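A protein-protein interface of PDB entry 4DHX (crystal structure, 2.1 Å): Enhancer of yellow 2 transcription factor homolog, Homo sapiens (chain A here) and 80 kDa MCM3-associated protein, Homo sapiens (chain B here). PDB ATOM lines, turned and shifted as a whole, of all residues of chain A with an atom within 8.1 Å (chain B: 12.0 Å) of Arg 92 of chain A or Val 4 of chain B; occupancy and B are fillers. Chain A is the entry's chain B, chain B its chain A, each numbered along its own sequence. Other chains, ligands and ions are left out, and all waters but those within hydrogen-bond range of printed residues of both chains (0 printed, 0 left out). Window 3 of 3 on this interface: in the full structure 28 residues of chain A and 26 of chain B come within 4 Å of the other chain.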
ATOM      1  N   LEU A  20       2.765   7.142 -14.397  1.00  0.00           N
ATOM      2  CA  LEU A  20       1.315   7.142 -14.241  1.00  0.00           C
ATOM      3  C   LEU A  20       0.735   8.469 -14.713  1.00  0.00           C
ATOM      4  O   LEU A  20      -0.321   8.509 -15.344  1.00  0.00           O
ATOM      5  CB  LEU A  20       0.938   6.904 -12.779  1.00  0.00           C
ATOM      6  CG  LEU A  20       1.124   5.478 -12.260  1.00  0.00           C
ATOM      7  CD1 LEU A  20       1.102   5.458 -10.742  1.00  0.00           C
ATOM      8  CD2 LEU A  20       0.043   4.569 -12.819  1.00  0.00           C
ATOM      9  N   LEU A  29      -7.511   6.620 -13.723  1.00  0.00           N
ATOM     10  CA  LEU A  29      -7.841   5.840 -12.537  1.00  0.00           C
ATOM     11  C   LEU A  29      -8.606   6.695 -11.537  1.00  0.00           C
ATOM     12  O   LEU A  29      -9.557   6.236 -10.906  1.00  0.00           O
ATOM     13  CB  LEU A  29      -6.568   5.307 -11.882  1.00  0.00           C
ATOM     14  CG  LEU A  29      -5.774   4.280 -12.690  1.00  0.00           C
ATOM     15  CD1 LEU A  29      -4.445   3.998 -12.013  1.00  0.00           C
ATOM     16  CD2 LEU A  29      -6.574   3.000 -12.860  1.00  0.00           C
ATOM     17  N   LYS A  85      -9.322  -3.483  -4.027  1.00  0.00           N
ATOM     18  CA  LYS A  85      -8.808  -4.696  -4.653  1.00  0.00           C
ATOM     19  C   LYS A  85      -8.659  -4.494  -6.158  1.00  0.00           C
ATOM     20  O   LYS A  85      -7.670  -4.918  -6.758  1.00  0.00           O
ATOM     21  CB  LYS A  85      -9.743  -5.874  -4.372  1.00  0.00           C
ATOM     22  CG  LYS A  85      -9.393  -7.150  -5.119  1.00  0.00           C
ATOM     23  CD  LYS A  85     -10.400  -8.251  -4.821  1.00  0.00           C
ATOM     24  CE  LYS A  85     -10.187  -9.472  -5.705  1.00  0.00           C
ATOM     25  NZ  LYS A  85      -8.880 -10.139  -5.451  1.00  0.00           N
ATOM     26  N   GLU A  86      -9.645  -3.840  -6.762  1.00  0.00           N
ATOM     27  CA  GLU A  86      -9.633  -3.595  -8.199  1.00  0.00           C
ATOM     28  C   GLU A  86      -8.565  -2.568  -8.566  1.00  0.00           C
ATOM     29  O   GLU A  86      -7.892  -2.698  -9.588  1.00  0.00           O
ATOM     30  CB  GLU A  86     -11.008  -3.118  -8.670  1.00  0.00           C
ATOM     31  CG  GLU A  86     -11.132  -2.983 -10.179  1.00  0.00           C
ATOM     32  CD  GLU A  86     -12.572  -2.849 -10.639  1.00  0.00           C
ATOM     33  OE1 GLU A  86     -13.464  -2.705  -9.775  1.00  0.00           O
ATOM     34  OE2 GLU A  86     -12.812  -2.893 -11.864  1.00  0.00           O
ATOM     35  N   LEU A  87      -8.409  -1.550  -7.726  1.00  0.00           N
ATOM     36  CA  LEU A  87      -7.398  -0.526  -7.953  1.00  0.00           C
ATOM     37  C   LEU A  87      -6.005  -1.149  -7.970  1.00  0.00           C
ATOM     38  O   LEU A  87      -5.232  -0.940  -8.904  1.00  0.00           O
ATOM     39  CB  LEU A  87      -7.474   0.551  -6.870  1.00  0.00           C
ATOM     40  CG  LEU A  87      -6.432   1.666  -6.989  1.00  0.00           C
ATOM     41  CD1 LEU A  87      -6.546   2.363  -8.338  1.00  0.00           C
ATOM     42  CD2 LEU A  87      -6.581   2.666  -5.851  1.00  0.00           C
ATOM     43  N   LEU A  88      -5.693  -1.918  -6.934  1.00  0.00           N
ATOM     44  CA  LEU A  88      -4.404  -2.591  -6.837  1.00  0.00           C
ATOM     45  C   LEU A  88      -4.111  -3.408  -8.093  1.00  0.00           C
ATOM     46  O   LEU A  88      -2.980  -3.427  -8.585  1.00  0.00           O
ATOM     47  CB  LEU A  88      -4.378  -3.499  -5.608  1.00  0.00           C
ATOM     48  CG  LEU A  88      -3.136  -4.378  -5.440  1.00  0.00           C
ATOM     49  CD1 LEU A  88      -1.870  -3.534  -5.408  1.00  0.00           C
ATOM     50  CD2 LEU A  88      -3.259  -5.213  -4.177  1.00  0.00           C
ATOM     51  N   GLN A  89      -5.134  -4.081  -8.611  1.00  0.00           N
ATOM     52  CA  GLN A  89      -4.978  -4.908  -9.801  1.00  0.00           C
ATOM     53  C   GLN A  89      -4.658  -4.058 -11.029  1.00  0.00           C
ATOM     54  O   GLN A  89      -3.877  -4.471 -11.891  1.00  0.00           O
ATOM     55  CB  GLN A  89      -6.245  -5.727 -10.052  1.00  0.00           C
ATOM     56  CG  GLN A  89      -6.158  -6.643 -11.262  1.00  0.00           C
ATOM     57  CD  GLN A  89      -5.025  -7.648 -11.152  1.00  0.00           C
ATOM     58  OE1 GLN A  89      -5.072  -8.564 -10.331  1.00  0.00           O
ATOM     59  NE2 GLN A  89      -3.997  -7.478 -11.977  1.00  0.00           N
ATOM     60  N   ARG A  90      -5.271  -2.881 -11.111  1.00  0.00           N
ATOM     61  CA  ARG A  90      -5.018  -1.963 -12.220  1.00  0.00           C
ATOM     62  C   ARG A  90      -3.577  -1.466 -12.175  1.00  0.00           C
ATOM     63  O   ARG A  90      -2.907  -1.380 -13.206  1.00  0.00           O
ATOM     64  CB  ARG A  90      -5.983  -0.774 -12.178  1.00  0.00           C
ATOM     65  CG  ARG A  90      -7.444  -1.135 -12.427  1.00  0.00           C
ATOM     66  CD  ARG A  90      -7.671  -1.636 -13.843  1.00  0.00           C
ATOM     67  NE  ARG A  90      -9.057  -2.049 -14.068  1.00  0.00           N
ATOM     68  CZ  ARG A  90      -9.967  -1.353 -14.750  1.00  0.00           C
ATOM     69  NH1 ARG A  90      -9.670  -0.185 -15.308  1.00  0.00           N
ATOM     70  NH2 ARG A  90     -11.193  -1.836 -14.881  1.00  0.00           N
ATOM     71  N   ILE A  91      -3.103  -1.149 -10.974  1.00  0.00           N
ATOM     72  CA  ILE A  91      -1.737  -0.674 -10.786  1.00  0.00           C
ATOM     73  C   ILE A  91      -0.730  -1.723 -11.250  1.00  0.00           C
ATOM     74  O   ILE A  91       0.223  -1.411 -11.963  1.00  0.00           O
ATOM     75  CB  ILE A  91      -1.461  -0.339  -9.307  1.00  0.00           C
ATOM     76  CG1 ILE A  91      -2.374   0.796  -8.831  1.00  0.00           C
ATOM     77  CG2 ILE A  91      -0.001   0.040  -9.106  1.00  0.00           C
ATOM     78  CD1 ILE A  91      -2.173   2.108  -9.561  1.00  0.00           C
ATOM     79  N   ARG A  92      -0.944  -2.968 -10.839  1.00  0.00           N
ATOM     80  CA  ARG A  92      -0.047  -4.056 -11.206  1.00  0.00           C
ATOM     81  C   ARG A  92      -0.047  -4.269 -12.715  1.00  0.00           C
ATOM     82  O   ARG A  92       1.007  -4.429 -13.326  1.00  0.00           O
ATOM     83  CB  ARG A  92      -0.447  -5.341 -10.481  1.00  0.00           C
ATOM     84  CG  ARG A  92      -0.108  -5.322  -8.999  1.00  0.00           C
ATOM     85  CD  ARG A  92      -0.748  -6.476  -8.244  1.00  0.00           C
ATOM     86  NE  ARG A  92      -0.222  -6.579  -6.887  1.00  0.00           N
ATOM     87  CZ  ARG A  92      -0.772  -7.294  -5.909  1.00  0.00           C
ATOM     88  NH1 ARG A  92      -1.888  -7.982  -6.118  1.00  0.00           N
ATOM     89  NH2 ARG A  92      -0.202  -7.313  -4.712  1.00  0.00           N
ATOM     90  N   THR A  93      -1.235  -4.263 -13.310  1.00  0.00           N
ATOM     91  CA  THR A  93      -1.365  -4.381 -14.758  1.00  0.00           C
ATOM     92  C   THR A  93      -0.585  -3.269 -15.452  1.00  0.00           C
ATOM     93  O   THR A  93       0.042  -3.491 -16.486  1.00  0.00           O
ATOM     94  CB  THR A  93      -2.839  -4.312 -15.197  1.00  0.00           C
ATOM     95  OG1 THR A  93      -3.537  -5.470 -14.722  1.00  0.00           O
ATOM     96  CG2 THR A  93      -2.950  -4.246 -16.716  1.00  0.00           C
ATOM     97  N   PHE A  94      -0.625  -2.074 -14.874  1.00  0.00           N
ATOM     98  CA  PHE A  94       0.064  -0.921 -15.446  1.00  0.00           C
ATOM     99  C   PHE A  94       1.582  -1.066 -15.356  1.00  0.00           C
ATOM    100  O   PHE A  94       2.299  -0.743 -16.304  1.00  0.00           O
ATOM    101  CB  PHE A  94      -0.380   0.366 -14.749  1.00  0.00           C
ATOM    102  CG  PHE A  94       0.433   1.569 -15.126  1.00  0.00           C
ATOM    103  CD1 PHE A  94       0.141   2.291 -16.271  1.00  0.00           C
ATOM    104  CD2 PHE A  94       1.491   1.982 -14.331  1.00  0.00           C
ATOM    105  CE1 PHE A  94       0.888   3.401 -16.619  1.00  0.00           C
ATOM    106  CE2 PHE A  94       2.243   3.090 -14.674  1.00  0.00           C
ATOM    107  CZ  PHE A  94       1.941   3.800 -15.819  1.00  0.00           C
ATOM    108  N   LEU A  95       2.071  -1.550 -14.219  1.00  0.00           N
ATOM    109  CA  LEU A  95       3.504  -1.749 -14.035  1.00  0.00           C
ATOM    110  C   LEU A  95       4.031  -2.810 -14.993  1.00  0.00           C
ATOM    111  O   LEU A  95       5.117  -2.669 -15.551  1.00  0.00           O
ATOM    112  CB  LEU A  95       3.814  -2.155 -12.593  1.00  0.00           C
ATOM    113  CG  LEU A  95       3.680  -1.063 -11.530  1.00  0.00           C
ATOM    114  CD1 LEU A  95       4.080  -1.604 -10.164  1.00  0.00           C
ATOM    115  CD2 LEU A  95       4.519   0.154 -11.889  1.00  0.00           C
ATOM    116  N   ALA A  96       3.251  -3.869 -15.182  1.00  0.00           N
ATOM    117  CA  ALA A  96       3.660  -4.981 -16.028  1.00  0.00           C
ATOM    118  C   ALA A  96       3.804  -4.565 -17.491  1.00  0.00           C
ATOM    119  O   ALA A  96       4.623  -5.123 -18.221  1.00  0.00           O
ATOM    120  CB  ALA A  96       2.667  -6.126 -15.902  1.00  0.00           C
ATOM    121  N   GLN A  97       3.015  -3.583 -17.919  1.00  0.00           N
ATOM    122  CA  GLN A  97       3.003  -3.180 -19.322  1.00  0.00           C
ATOM    123  C   GLN A  97       3.955  -2.019 -19.617  1.00  0.00           C
ATOM    124  O   GLN A  97       4.295  -1.774 -20.773  1.00  0.00           O
ATOM    125  CB  GLN A  97       1.581  -2.829 -19.775  1.00  0.00           C
ATOM    126  CG  GLN A  97       1.014  -1.555 -19.172  1.00  0.00           C
ATOM    127  CD  GLN A  97      -0.393  -1.258 -19.660  1.00  0.00           C
ATOM    128  OE1 GLN A  97      -0.994  -2.058 -20.377  1.00  0.00           O
ATOM    129  NE2 GLN A  97      -0.924  -0.103 -19.272  1.00  0.00           N
ATOM    130  N   HIS A  98       4.386  -1.310 -18.579  1.00  0.00           N
ATOM    131  CA  HIS A  98       5.340  -0.218 -18.754  1.00  0.00           C
ATOM    132  C   HIS A  98       6.705  -0.536 -18.144  1.00  0.00           C
ATOM    133  O   HIS A  98       7.599   0.312 -18.130  1.00  0.00           O
ATOM    134  CB  HIS A  98       4.784   1.081 -18.167  1.00  0.00           C
ATOM    135  CG  HIS A  98       3.694   1.694 -18.989  1.00  0.00           C
ATOM    136  ND1 HIS A  98       2.358   1.441 -18.764  1.00  0.00           N
ATOM    137  CD2 HIS A  98       3.743   2.544 -20.041  1.00  0.00           C
ATOM    138  CE1 HIS A  98       1.631   2.111 -19.641  1.00  0.00           C
ATOM    139  NE2 HIS A  98       2.449   2.788 -20.427  1.00  0.00           N
ATOM    140  N   ALA A  99       6.866  -1.758 -17.644  1.00  0.00           N
ATOM    141  CA  ALA A  99       8.153  -2.200 -17.121  1.00  0.00           C
ATOM    142  C   ALA A  99       8.249  -3.720 -17.142  1.00  0.00           C
ATOM    143  O   ALA A  99       8.352  -4.359 -16.095  1.00  0.00           O
ATOM    144  CB  ALA A  99       8.361  -1.674 -15.708  1.00  0.00           C
ATOM    145  N   LEU B   3       3.034 -14.573  -7.407  1.00  0.00           N
ATOM    146  CA  LEU B   3       4.171 -14.262  -6.548  1.00  0.00           C
ATOM    147  C   LEU B   3       4.520 -12.779  -6.614  1.00  0.00           C
ATOM    148  O   LEU B   3       5.235 -12.339  -7.515  1.00  0.00           O
ATOM    149  CB  LEU B   3       5.387 -15.096  -6.952  1.00  0.00           C
ATOM    150  CG  LEU B   3       6.689 -14.778  -6.211  1.00  0.00           C
ATOM    151  CD1 LEU B   3       6.529 -15.015  -4.717  1.00  0.00           C
ATOM    152  CD2 LEU B   3       7.839 -15.600  -6.770  1.00  0.00           C
ATOM    153  N   VAL B   4       4.014 -12.012  -5.656  1.00  0.00           N
ATOM    154  CA  VAL B   4       4.328 -10.590  -5.576  1.00  0.00           C
ATOM    155  C   VAL B   4       5.641 -10.389  -4.827  1.00  0.00           C
ATOM    156  O   VAL B   4       5.726 -10.639  -3.624  1.00  0.00           O
ATOM    157  CB  VAL B   4       3.206  -9.807  -4.872  1.00  0.00           C
ATOM    158  CG1 VAL B   4       3.633  -8.368  -4.620  1.00  0.00           C
ATOM    159  CG2 VAL B   4       1.932  -9.852  -5.703  1.00  0.00           C
ATOM    160  N   LEU B   5       6.663  -9.940  -5.547  1.00  0.00           N
ATOM    161  CA  LEU B   5       7.987  -9.754  -4.967  1.00  0.00           C
ATOM    162  C   LEU B   5       7.997  -8.628  -3.944  1.00  0.00           C
ATOM    163  O   LEU B   5       8.356  -8.828  -2.784  1.00  0.00           O
ATOM    164  CB  LEU B   5       9.013  -9.452  -6.061  1.00  0.00           C
ATOM    165  CG  LEU B   5       9.563 -10.661  -6.821  1.00  0.00           C
ATOM    166  CD1 LEU B   5      10.343 -11.570  -5.886  1.00  0.00           C
ATOM    167  CD2 LEU B   5       8.442 -11.422  -7.498  1.00  0.00           C
ATOM    168  N   SER B   6       7.593  -7.441  -4.385  1.00  0.00           N
ATOM    169  CA  SER B   6       7.668  -6.253  -3.549  1.00  0.00           C
ATOM    170  C   SER B   6       6.284  -5.740  -3.181  1.00  0.00           C
ATOM    171  O   SER B   6       5.293  -6.060  -3.836  1.00  0.00           O
ATOM    172  CB  SER B   6       8.448  -5.154  -4.272  1.00  0.00           C
ATOM    173  OG  SER B   6       8.579  -4.003  -3.459  1.00  0.00           O
ATOM    174  N   GLU B   7       6.233  -4.938  -2.125  1.00  0.00           N
ATOM    175  CA  GLU B   7       4.996  -4.299  -1.694  1.00  0.00           C
ATOM    176  C   GLU B   7       4.930  -2.883  -2.255  1.00  0.00           C
ATOM    177  O   GLU B   7       4.248  -2.014  -1.710  1.00  0.00           O
ATOM    178  CB  GLU B   7       4.907  -4.277  -0.166  1.00  0.00           C
ATOM    179  CG  GLU B   7       6.048  -3.535   0.520  1.00  0.00           C
ATOM    180  CD  GLU B   7       6.164  -3.874   1.993  1.00  0.00           C
ATOM    181  OE1 GLU B   7       5.228  -4.495   2.536  1.00  0.00           O
ATOM    182  OE2 GLU B   7       7.198  -3.531   2.604  1.00  0.00           O
ATOM    183  N   LEU B   8       5.641  -2.661  -3.357  1.00  0.00           N
ATOM    184  CA  LEU B   8       5.687  -1.351  -3.991  1.00  0.00           C
ATOM    185  C   LEU B   8       4.350  -1.013  -4.642  1.00  0.00           C
ATOM    186  O   LEU B   8       3.870   0.117  -4.541  1.00  0.00           O
ATOM    187  CB  LEU B   8       6.809  -1.316  -5.030  1.00  0.00           C
ATOM    188  CG  LEU B   8       7.035   0.013  -5.752  1.00  0.00           C
ATOM    189  CD1 LEU B   8       8.515   0.210  -6.041  1.00  0.00           C
ATOM    190  CD2 LEU B   8       6.233   0.070  -7.041  1.00  0.00           C
ATOM    191  N   SER B   9       3.748  -1.997  -5.304  1.00  0.00           N
ATOM    192  CA  SER B   9       2.459  -1.800  -5.951  1.00  0.00           C
ATOM    193  C   SER B   9       1.358  -1.608  -4.915  1.00  0.00           C
ATOM    194  O   SER B   9       0.417  -0.844  -5.132  1.00  0.00           O
ATOM    195  CB  SER B   9       2.124  -2.983  -6.860  1.00  0.00           C
ATOM    196  OG  SER B   9       2.159  -4.212  -6.155  1.00  0.00           O
ATOM    197  N   GLN B  10       1.471  -2.311  -3.794  1.00  0.00           N
ATOM    198  CA  GLN B  10       0.525  -2.147  -2.697  1.00  0.00           C
ATOM    199  C   GLN B  10       0.582  -0.717  -2.171  1.00  0.00           C
ATOM    200  O   GLN B  10      -0.448  -0.093  -1.927  1.00  0.00           O
ATOM    201  CB  GLN B  10       0.829  -3.134  -1.567  1.00  0.00           C
ATOM    202  CG  GLN B  10      -0.079  -3.003  -0.349  1.00  0.00           C
ATOM    203  CD  GLN B  10      -1.493  -3.484  -0.613  1.00  0.00           C
ATOM    204  OE1 GLN B  10      -1.942  -3.535  -1.758  1.00  0.00           O
ATOM    205  NE2 GLN B  10      -2.201  -3.850   0.449  1.00  0.00           N
ATOM    206  N   GLY B  11       1.798  -0.205  -2.004  1.00  0.00           N
ATOM    207  CA  GLY B  11       1.998   1.143  -1.509  1.00  0.00           C
ATOM    208  C   GLY B  11       1.428   2.196  -2.439  1.00  0.00           C
ATOM    209  O   GLY B  11       0.888   3.205  -1.990  1.00  0.00           O
ATOM    210  N   LEU B  12       1.549   1.961  -3.742  1.00  0.00           N
ATOM    211  CA  LEU B  12       1.055   2.904  -4.739  1.00  0.00           C
ATOM    212  C   LEU B  12      -0.471   2.945  -4.749  1.00  0.00           C
ATOM    213  O   LEU B  12      -1.070   4.012  -4.888  1.00  0.00           O
ATOM    214  CB  LEU B  12       1.584   2.537  -6.128  1.00  0.00           C
ATOM    215  CG  LEU B  12       3.051   2.882  -6.389  1.00  0.00           C
ATOM    216  CD1 LEU B  12       3.564   2.151  -7.620  1.00  0.00           C
ATOM    217  CD2 LEU B  12       3.226   4.385  -6.552  1.00  0.00           C
ATOM    218  N   ALA B  13      -1.094   1.781  -4.599  1.00  0.00           N
ATOM    219  CA  ALA B  13      -2.549   1.695  -4.568  1.00  0.00           C
ATOM    220  C   ALA B  13      -3.097   2.359  -3.308  1.00  0.00           C
ATOM    221  O   ALA B  13      -4.154   2.989  -3.334  1.00  0.00           O
ATOM    222  CB  ALA B  13      -2.994   0.243  -4.637  1.00  0.00           C
ATOM    223  N   VAL B  14      -2.367   2.220  -2.206  1.00  0.00           N
ATOM    224  CA  VAL B  14      -2.791   2.792  -0.934  1.00  0.00           C
ATOM    225  C   VAL B  14      -2.682   4.315  -0.946  1.00  0.00           C
ATOM    226  O   VAL B  14      -3.581   5.013  -0.476  1.00  0.00           O
ATOM    227  CB  VAL B  14      -1.964   2.228   0.233  1.00  0.00           C
ATOM    228  CG1 VAL B  14      -2.164   3.064   1.491  1.00  0.00           C
ATOM    229  CG2 VAL B  14      -2.346   0.779   0.492  1.00  0.00           C
ATOM    230  N   LEU B  16      -2.486   6.318  -3.710  1.00  0.00           N
ATOM    231  CA  LEU B  16      -3.378   6.849  -4.731  1.00  0.00           C
ATOM    232  C   LEU B  16      -4.809   6.903  -4.212  1.00  0.00           C
ATOM    233  O   LEU B  16      -5.500   7.907  -4.377  1.00  0.00           O
ATOM    234  CB  LEU B  16      -3.310   5.990  -5.995  1.00  0.00           C
ATOM    235  CG  LEU B  16      -4.335   6.315  -7.083  1.00  0.00           C
ATOM    236  CD1 LEU B  16      -4.304   7.794  -7.440  1.00  0.00           C
ATOM    237  CD2 LEU B  16      -4.088   5.465  -8.320  1.00  0.00           C
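The side-chain hydroxyl of Ser 9 of chain B lies within hydrogen-bond range of the guanidinium group of Arg 92 of chain A, at 3.4 Å.
Among the printed residues, pairs that only touch across the chains: Leu 88 of chain A with Gln 10 of chain B, Arg 92 of chain A with Val 4 of chain B, Leu 87 of chain A with Ala 13 of chain B, Leu 88 of chain A with Ser 9 of chain B, Leu 88 of chain A with Ala 13 of chain B, Leu 87 of chain A with Leu 16 of chain B and Leu 29 of chain A with Leu 16 of chain B.
Arg 92 of chain A touches two residues of chain B.
Of chain A, only Arg 92 (3.5 Å) comes within 4 Å of Val 4 of chain B.
Of chain B, only Ser 9, Gln 10 and Ala 13 come within 4 Å of Leu 88 of chain A.
No residue of chain B comes within 4 Å of Ile 91 of chain A.
No residue of chain B comes within 4 Å of Thr 93 of chain A.
No residue of chain B comes within 4 Å of Leu 95 of chain A.
No residue of chain B comes within 4 Å of Ala 96 of chain A.
Printed residues of chain B within 4 Å of Leu 29 of chain A: Leu 16 (3.99 Å).
Printed residues of chain B within 4 Å of Leu 87 of chain A: Ala 13 and Leu 16.
Printed residues of chain A within 4 Å of Ala 13 of chain B: Leu 87 (3.5 Å) and Leu 88 (3.9 Å).
Printed residues of chain A within 4 Å of Leu 16 of chain B: Leu 29 and Leu 87.
Val 14 of chain B touches none of the printed residues of chain A.
The nearest printed residue of chain A that does not touch Leu 16 of chain B is Ile 91 of chain A (4.1 Å).
Of the 17 printed residues of chain A, 4 touch a printed residue of chain B.
Among the printed residues, no Asp or Glu carboxylate lies within 4 Å of a Lys or Arg side-chain nitrogen of the other chain.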
